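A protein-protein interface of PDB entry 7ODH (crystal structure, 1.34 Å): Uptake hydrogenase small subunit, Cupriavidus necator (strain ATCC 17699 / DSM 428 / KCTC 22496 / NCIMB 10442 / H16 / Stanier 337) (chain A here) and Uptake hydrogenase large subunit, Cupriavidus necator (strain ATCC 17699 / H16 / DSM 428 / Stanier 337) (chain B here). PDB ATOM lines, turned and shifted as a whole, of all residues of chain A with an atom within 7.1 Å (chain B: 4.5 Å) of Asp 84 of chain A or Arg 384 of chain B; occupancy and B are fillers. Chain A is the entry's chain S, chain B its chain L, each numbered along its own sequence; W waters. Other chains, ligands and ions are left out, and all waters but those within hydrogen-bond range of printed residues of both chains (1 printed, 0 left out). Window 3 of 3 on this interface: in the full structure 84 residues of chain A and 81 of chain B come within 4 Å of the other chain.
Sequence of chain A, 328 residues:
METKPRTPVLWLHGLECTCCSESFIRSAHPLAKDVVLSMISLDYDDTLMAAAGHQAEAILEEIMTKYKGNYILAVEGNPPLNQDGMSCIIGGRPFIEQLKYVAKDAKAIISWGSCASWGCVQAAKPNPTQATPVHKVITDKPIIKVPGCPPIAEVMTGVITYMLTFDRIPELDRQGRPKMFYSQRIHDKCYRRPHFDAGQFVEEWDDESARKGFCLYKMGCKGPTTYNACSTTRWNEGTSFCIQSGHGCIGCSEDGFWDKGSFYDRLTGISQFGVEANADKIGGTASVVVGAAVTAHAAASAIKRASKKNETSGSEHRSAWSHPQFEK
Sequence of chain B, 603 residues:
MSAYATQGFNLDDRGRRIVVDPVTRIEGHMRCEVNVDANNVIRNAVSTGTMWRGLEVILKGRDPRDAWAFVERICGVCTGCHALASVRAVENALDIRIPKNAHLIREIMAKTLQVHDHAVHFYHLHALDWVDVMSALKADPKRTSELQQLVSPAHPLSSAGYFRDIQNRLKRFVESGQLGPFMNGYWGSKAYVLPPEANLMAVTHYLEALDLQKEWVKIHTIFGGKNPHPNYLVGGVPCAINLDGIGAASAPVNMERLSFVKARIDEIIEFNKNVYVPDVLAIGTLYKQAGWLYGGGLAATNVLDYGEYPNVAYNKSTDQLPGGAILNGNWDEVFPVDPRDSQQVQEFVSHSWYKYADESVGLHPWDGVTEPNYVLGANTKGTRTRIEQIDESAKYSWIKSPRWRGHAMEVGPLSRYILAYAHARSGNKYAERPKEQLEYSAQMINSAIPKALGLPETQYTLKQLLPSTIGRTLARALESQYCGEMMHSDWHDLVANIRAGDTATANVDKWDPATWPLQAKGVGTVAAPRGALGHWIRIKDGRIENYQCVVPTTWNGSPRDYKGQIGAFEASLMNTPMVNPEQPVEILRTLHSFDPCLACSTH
O of Gln 83 of chain A touches CD2 of Tyr 374 of chain B, at 3.9 Å.
Asp 84 of chain A touches Thr 385 of chain B (O to CG2, 3.7 Å).
Met 86 of chain A touches Tyr 374 of chain B (CE to OH, 3.3 Å).
Thr 385 of chain B touches Met 86 of chain A (CA to SD, 3.8 Å).
Gly 92 of chain A touches Thr 385 of chain B (O to O, 3.6 Å).
Arg 386 of chain B touches Gly 92 of chain A.
CA of Arg 93 of chain A touches O of Thr 385 of chain B, at 3.5 Å.
Thr 385 of chain B touches Pro 94 of chain A (O to CD, 3.2 Å).
Of the 14 printed residues of chain A, 6 touch a printed residue of chain B.
Printed residues of chain A that touch a printed residue of chain B: Gln 83, Asp 84, Met 86, Gly 92, Arg 93 and Pro 94.
The side-chain hydroxyl of Tyr 374 of chain B lies within hydrogen-bond range of the backbone carbonyl oxygen of Arg 384 of chain B, at 2.7 Å.
OG1 of Thr 383 of chain B lies close to N of Thr 385 of chain B (3.4 Å).
N of Arg 386 of chain B is in hydrogen-bond range of OG1 of Thr 383 of chain B, at 3.0 Å.
The side-chain hydroxyl (OG) of Ser 87 of chain A lies within hydrogen-bond range of the side-chain amide oxygen (OE1) of Gln 83 of chain A, 2.8 Å away.
Printed residues of chain B within 4 Å of Gln 83 of chain A: Tyr 374.
Asp 84 of chain A touches two residues of chain B.
Printed residues of chain A within 4 Å of Tyr 374 of chain B: Gln 83 (3.9 Å) and Met 86 (3.3 Å).
Arg 384 of chain B touches two residues of chain A.
The nearest printed residue of chain B that does not touch Asp 84 of chain A is Tyr 374 of chain B (5.4 Å).
NH2 of Arg 384 of chain B lies within salt-bridge range of OD2 of Asp 84 of chain A (2.8 Å).
SD of Met 86 of chain A lies close to O of Arg 384 of chain B, 3.8 Å away.
The guanidinium group (NH1) of Arg 386 of chain B sits close to the guanidinium group (NH1) of Arg 93 of chain A, at 3.2 Å.
Water W1 lies within hydrogen-bond range of O of Thr 385 of chain B (2.7 Å), OE1 of Glu 97 of chain A (2.7 Å) and NE of Arg 386 of chain B (3.2 Å).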
ATOM      1  N   PRO A  80      -6.792  17.215   1.501  1.00  0.00           N
ATOM      2  CA  PRO A  80      -8.103  17.034   0.887  1.00  0.00           C
ATOM      3  C   PRO A  80      -8.742  18.377   0.519  1.00  0.00           C
ATOM      4  O   PRO A  80      -8.643  19.311   1.305  1.00  0.00           O
ATOM      5  CB  PRO A  80      -8.897  16.349   2.001  1.00  0.00           C
ATOM      6  CG  PRO A  80      -8.325  16.933   3.272  1.00  0.00           C
ATOM      7  CD  PRO A  80      -6.862  17.187   2.971  1.00  0.00           C
ATOM      8  N   LEU A  81      -9.407  18.445  -0.634  1.00  0.00           N
ATOM      9  CA  LEU A  81     -10.106  19.683  -1.071  1.00  0.00           C
ATOM     10  C   LEU A  81     -11.608  19.591  -0.775  1.00  0.00           C
ATOM     11  O   LEU A  81     -12.260  20.647  -0.773  1.00  0.00           O
ATOM     12  CB  LEU A  81      -9.841  19.940  -2.557  1.00  0.00           C
ATOM     13  CG  LEU A  81      -8.376  20.148  -2.934  1.00  0.00           C
ATOM     14  CD1 LEU A  81      -8.248  20.554  -4.393  1.00  0.00           C
ATOM     15  CD2 LEU A  81      -7.706  21.177  -2.035  1.00  0.00           C
ATOM     16  N   ASN A  82     -12.145  18.396  -0.525  1.00  0.00           N
ATOM     17  CA  ASN A  82     -13.572  18.231  -0.144  1.00  0.00           C
ATOM     18  C   ASN A  82     -13.724  18.509   1.355  1.00  0.00           C
ATOM     19  O   ASN A  82     -12.699  18.727   2.044  1.00  0.00           O
ATOM     20  CB  ASN A  82     -14.120  16.863  -0.555  1.00  0.00           C
ATOM     21  CG  ASN A  82     -14.385  16.743  -2.042  1.00  0.00           C
ATOM     22  OD1 ASN A  82     -14.353  17.736  -2.772  1.00  0.00           O
ATOM     23  ND2 ASN A  82     -14.624  15.524  -2.502  1.00  0.00           N
ATOM     24  N   GLN A  83     -14.969  18.549   1.830  1.00  0.00           N
ATOM     25  CA  GLN A  83     -15.314  18.857   3.243  1.00  0.00           C
ATOM     26  C   GLN A  83     -14.687  20.203   3.653  1.00  0.00           C
ATOM     27  O   GLN A  83     -14.344  20.356   4.833  1.00  0.00           O
ATOM     28  CB  GLN A  83     -14.839  17.714   4.149  1.00  0.00           C
ATOM     29  CG  GLN A  83     -15.493  16.368   3.845  1.00  0.00           C
ATOM     30  CD  GLN A  83     -14.854  15.593   2.712  1.00  0.00           C
ATOM     31  OE1 GLN A  83     -13.635  15.581   2.527  1.00  0.00           O
ATOM     32  NE2 GLN A  83     -15.685  14.901   1.949  1.00  0.00           N
ATOM     33  N   ASP A  84     -14.559  21.152   2.715  1.00  0.00           N
ATOM     34  CA  ASP A  84     -13.934  22.487   2.937  1.00  0.00           C
ATOM     35  C   ASP A  84     -12.523  22.311   3.515  1.00  0.00           C
ATOM     36  O   ASP A  84     -12.059  23.204   4.241  1.00  0.00           O
ATOM     37  CB  ASP A  84     -14.816  23.365   3.828  1.00  0.00           C
ATOM     38  CG  ASP A  84     -16.010  23.926   3.089  1.00  0.00           C
ATOM     39  OD1 ASP A  84     -15.797  24.495   1.999  1.00  0.00           O
ATOM     40  OD2 ASP A  84     -17.137  23.771   3.593  1.00  0.00           O
ATOM     41  N   GLY A  85     -11.859  21.201   3.182  1.00  0.00           N
ATOM     42  CA  GLY A  85     -10.496  20.894   3.652  1.00  0.00           C
ATOM     43  C   GLY A  85     -10.465  20.322   5.063  1.00  0.00           C
ATOM     44  O   GLY A  85      -9.369  19.990   5.535  1.00  0.00           O
ATOM     45  N   MET A  86     -11.618  20.165   5.712  1.00  0.00           N
ATOM     46  CA  MET A  86     -11.692  19.806   7.150  1.00  0.00           C
ATOM     47  C   MET A  86     -11.852  18.290   7.322  1.00  0.00           C
ATOM     48  O   MET A  86     -12.069  17.837   8.450  1.00  0.00           O
ATOM     49  CB  MET A  86     -12.835  20.562   7.829  1.00  0.00           C
ATOM     50  CG  MET A  86     -12.682  22.069   7.729  1.00  0.00           C
ATOM     51  SD  MET A  86     -11.218  22.708   8.598  1.00  0.00           S
ATOM     52  CE  MET A  86     -11.804  22.685  10.292  1.00  0.00           C
ATOM     53  N   SER A  87     -11.619  17.516   6.265  1.00  0.00           N
ATOM     54  CA  SER A  87     -11.281  16.073   6.393  1.00  0.00           C
ATOM     55  C   SER A  87      -9.798  15.909   6.771  1.00  0.00           C
ATOM     56  O   SER A  87      -9.356  14.770   6.978  1.00  0.00           O
ATOM     57  CB  SER A  87     -11.652  15.309   5.150  1.00  0.00           C
ATOM     58  OG  SER A  87     -11.349  16.056   3.990  1.00  0.00           O
ATOM     59  N   ILE A  89      -7.683  18.273   9.632  1.00  0.00           N
ATOM     60  CA  ILE A  89      -7.691  19.491  10.484  1.00  0.00           C
ATOM     61  C   ILE A  89      -6.404  19.512  11.307  1.00  0.00           C
ATOM     62  O   ILE A  89      -6.118  18.517  11.979  1.00  0.00           O
ATOM     63  CB  ILE A  89      -8.934  19.514  11.392  1.00  0.00           C
ATOM     64  CG1 ILE A  89     -10.236  19.395  10.591  1.00  0.00           C
ATOM     65  CG2 ILE A  89      -8.912  20.757  12.266  1.00  0.00           C
ATOM     66  CD1 ILE A  89     -11.450  19.046  11.430  1.00  0.00           C
ATOM     67  N   GLY A  92      -7.267  23.375  14.361  1.00  0.00           N
ATOM     68  CA  GLY A  92      -8.635  23.847  14.070  1.00  0.00           C
ATOM     69  C   GLY A  92      -8.801  24.386  12.656  1.00  0.00           C
ATOM     70  O   GLY A  92      -9.888  24.901  12.360  1.00  0.00           O
ATOM     71  N   ARG A  93      -7.794  24.251  11.790  1.00  0.00           N
ATOM     72  CA  ARG A  93      -7.816  24.820  10.419  1.00  0.00           C
ATOM     73  C   ARG A  93      -7.508  23.719   9.410  1.00  0.00           C
ATOM     74  O   ARG A  93      -6.903  22.702   9.747  1.00  0.00           O
ATOM     75  CB  ARG A  93      -6.806  25.964  10.306  1.00  0.00           C
ATOM     76  CG  ARG A  93      -7.041  27.091  11.299  1.00  0.00           C
ATOM     77  CD  ARG A  93      -6.038  28.211  11.128  1.00  0.00           C
ATOM     78  NE  ARG A  93      -6.079  29.156  12.233  1.00  0.00           N
ATOM     79  CZ  ARG A  93      -5.498  30.351  12.224  1.00  0.00           C
ATOM     80  NH1 ARG A  93      -4.823  30.758  11.160  1.00  0.00           N
ATOM     81  NH2 ARG A  93      -5.599  31.138  13.280  1.00  0.00           N
ATOM     82  N   PRO A  94      -7.888  23.887   8.127  1.00  0.00           N
ATOM     83  CA  PRO A  94      -7.552  22.889   7.119  1.00  0.00           C
ATOM     84  C   PRO A  94      -6.037  22.712   6.993  1.00  0.00           C
ATOM     85  O   PRO A  94      -5.305  23.693   7.012  1.00  0.00           O
ATOM     86  CB  PRO A  94      -8.111  23.444   5.807  1.00  0.00           C
ATOM     87  CG  PRO A  94      -9.096  24.514   6.212  1.00  0.00           C
ATOM     88  CD  PRO A  94      -8.651  25.015   7.572  1.00  0.00           C
ATOM     89  N   ILE A  96      -4.421  22.172   4.360  1.00  0.00           N
ATOM     90  CA  ILE A  96      -3.917  22.883   3.149  1.00  0.00           C
ATOM     91  C   ILE A  96      -3.392  24.270   3.547  1.00  0.00           C
ATOM     92  O   ILE A  96      -2.463  24.751   2.892  1.00  0.00           O
ATOM     93  CB  ILE A  96      -4.981  22.972   2.043  1.00  0.00           C
ATOM     94  CG1 ILE A  96      -4.330  23.325   0.703  1.00  0.00           C
ATOM     95  CG2 ILE A  96      -6.080  23.953   2.420  1.00  0.00           C
ATOM     96  CD1 ILE A  96      -5.234  23.137  -0.482  1.00  0.00           C
ATOM     97  N   GLU A  97      -3.964  24.898   4.578  1.00  0.00           N
ATOM     98  CA  GLU A  97      -3.530  26.246   5.034  1.00  0.00           C
ATOM     99  C   GLU A  97      -2.142  26.139   5.677  1.00  0.00           C
ATOM    100  O   GLU A  97      -1.297  27.009   5.419  1.00  0.00           O
ATOM    101  CB  GLU A  97      -4.574  26.848   5.970  1.00  0.00           C
ATOM    102  CG  GLU A  97      -5.855  27.216   5.249  1.00  0.00           C
ATOM    103  CD  GLU A  97      -6.884  27.967   6.074  1.00  0.00           C
ATOM    104  OE1 GLU A  97      -6.592  28.275   7.252  1.00  0.00           O
ATOM    105  OE2 GLU A  97      -7.977  28.242   5.531  1.00  0.00           O
ATOM    106  N   TYR B 374     -19.742  16.622   7.450  1.00  0.00           N
ATOM    107  CA  TYR B 374     -18.935  17.588   8.226  1.00  0.00           C
ATOM    108  C   TYR B 374     -19.807  18.814   8.513  1.00  0.00           C
ATOM    109  O   TYR B 374     -20.093  19.602   7.588  1.00  0.00           O
ATOM    110  CB  TYR B 374     -17.636  17.969   7.517  1.00  0.00           C
ATOM    111  CG  TYR B 374     -16.871  19.003   8.298  1.00  0.00           C
ATOM    112  CD1 TYR B 374     -16.297  18.689   9.521  1.00  0.00           C
ATOM    113  CD2 TYR B 374     -16.837  20.323   7.886  1.00  0.00           C
ATOM    114  CE1 TYR B 374     -15.645  19.648  10.279  1.00  0.00           C
ATOM    115  CE2 TYR B 374     -16.209  21.300   8.643  1.00  0.00           C
ATOM    116  CZ  TYR B 374     -15.606  20.962   9.840  1.00  0.00           C
ATOM    117  OH  TYR B 374     -14.976  21.917  10.585  1.00  0.00           O
ATOM    118  N   VAL B 375     -20.253  18.936   9.763  1.00  0.00           N
ATOM    119  CA  VAL B 375     -21.168  20.010  10.236  1.00  0.00           C
ATOM    120  C   VAL B 375     -20.858  20.256  11.713  1.00  0.00           C
ATOM    121  O   VAL B 375     -20.668  19.267  12.447  1.00  0.00           O
ATOM    122  CB  VAL B 375     -22.643  19.625  10.001  1.00  0.00           C
ATOM    123  CG1 VAL B 375     -23.017  18.317  10.675  1.00  0.00           C
ATOM    124  CG2 VAL B 375     -23.584  20.734  10.423  1.00  0.00           C
ATOM    125  N   LEU B 376     -20.797  21.524  12.121  1.00  0.00           N
ATOM    126  CA  LEU B 376     -20.414  21.920  13.499  1.00  0.00           C
ATOM    127  C   LEU B 376     -21.648  22.395  14.262  1.00  0.00           C
ATOM    128  O   LEU B 376     -22.550  22.998  13.642  1.00  0.00           O
ATOM    129  CB  LEU B 376     -19.347  23.013  13.446  1.00  0.00           C
ATOM    130  CG  LEU B 376     -18.053  22.652  12.719  1.00  0.00           C
ATOM    131  CD1 LEU B 376     -17.020  23.747  12.917  1.00  0.00           C
ATOM    132  CD2 LEU B 376     -17.501  21.306  13.176  1.00  0.00           C
ATOM    133  N   THR B 383     -15.305  29.225  13.281  1.00  0.00           N
ATOM    134  CA  THR B 383     -15.991  28.991  11.990  1.00  0.00           C
ATOM    135  C   THR B 383     -15.749  27.552  11.536  1.00  0.00           C
ATOM    136  O   THR B 383     -14.899  26.852  12.133  1.00  0.00           O
ATOM    137  CB  THR B 383     -15.497  29.962  10.911  1.00  0.00           C
ATOM    138  OG1 THR B 383     -14.171  29.562  10.563  1.00  0.00           O
ATOM    139  CG2 THR B 383     -15.516  31.408  11.353  1.00  0.00           C
ATOM    140  N   ARG B 384     -16.430  27.160  10.467  1.00  0.00           N
ATOM    141  CA  ARG B 384     -16.313  25.816   9.856  1.00  0.00           C
ATOM    142  C   ARG B 384     -14.854  25.501   9.511  1.00  0.00           C
ATOM    143  O   ARG B 384     -14.513  24.318   9.498  1.00  0.00           O
ATOM    144  CB  ARG B 384     -17.188  25.737   8.606  1.00  0.00           C
ATOM    145  CG  ARG B 384     -18.611  25.285   8.892  1.00  0.00           C
ATOM    146  CD  ARG B 384     -19.443  25.265   7.625  1.00  0.00           C
ATOM    147  NE  ARG B 384     -18.907  24.388   6.586  1.00  0.00           N
ATOM    148  CZ  ARG B 384     -19.116  23.070   6.502  1.00  0.00           C
ATOM    149  NH1 ARG B 384     -19.839  22.440   7.412  1.00  0.00           N
ATOM    150  NH2 ARG B 384     -18.604  22.384   5.495  1.00  0.00           N
ATOM    151  N   THR B 385     -14.031  26.498   9.184  1.00  0.00           N
ATOM    152  CA  THR B 385     -12.627  26.278   8.743  1.00  0.00           C
ATOM    153  C   THR B 385     -11.637  26.922   9.719  1.00  0.00           C
ATOM    154  O   THR B 385     -10.437  26.947   9.411  1.00  0.00           O
ATOM    155  CB  THR B 385     -12.414  26.782   7.311  1.00  0.00           C
ATOM    156  OG1 THR B 385     -12.755  28.167   7.272  1.00  0.00           O
ATOM    157  CG2 THR B 385     -13.230  26.006   6.301  1.00  0.00           C
ATOM    158  N   ARG B 386     -12.101  27.388  10.873  1.00  0.00           N
ATOM    159  CA  ARG B 386     -11.208  27.956  11.913  1.00  0.00           C
ATOM    160  C   ARG B 386     -11.846  27.738  13.278  1.00  0.00           C
ATOM    161  O   ARG B 386     -12.428  28.680  13.838  1.00  0.00           O
ATOM    162  CB  ARG B 386     -10.913  29.432  11.649  1.00  0.00           C
ATOM    163  CG  ARG B 386      -9.731  29.957  12.451  1.00  0.00           C
ATOM    164  CD  ARG B 386      -9.322  31.360  12.050  1.00  0.00           C
ATOM    165  NE  ARG B 386      -8.850  31.416  10.671  1.00  0.00           N
ATOM    166  CZ  ARG B 386      -7.838  32.162  10.237  1.00  0.00           C
ATOM    167  NH1 ARG B 386      -7.153  32.924  11.077  1.00  0.00           N
ATOM    168  NH2 ARG B 386      -7.503  32.133   8.958  1.00  0.00           N
HETATM  169  O   HOH W   1      -8.825  28.973   8.638  1.00  0.00           O
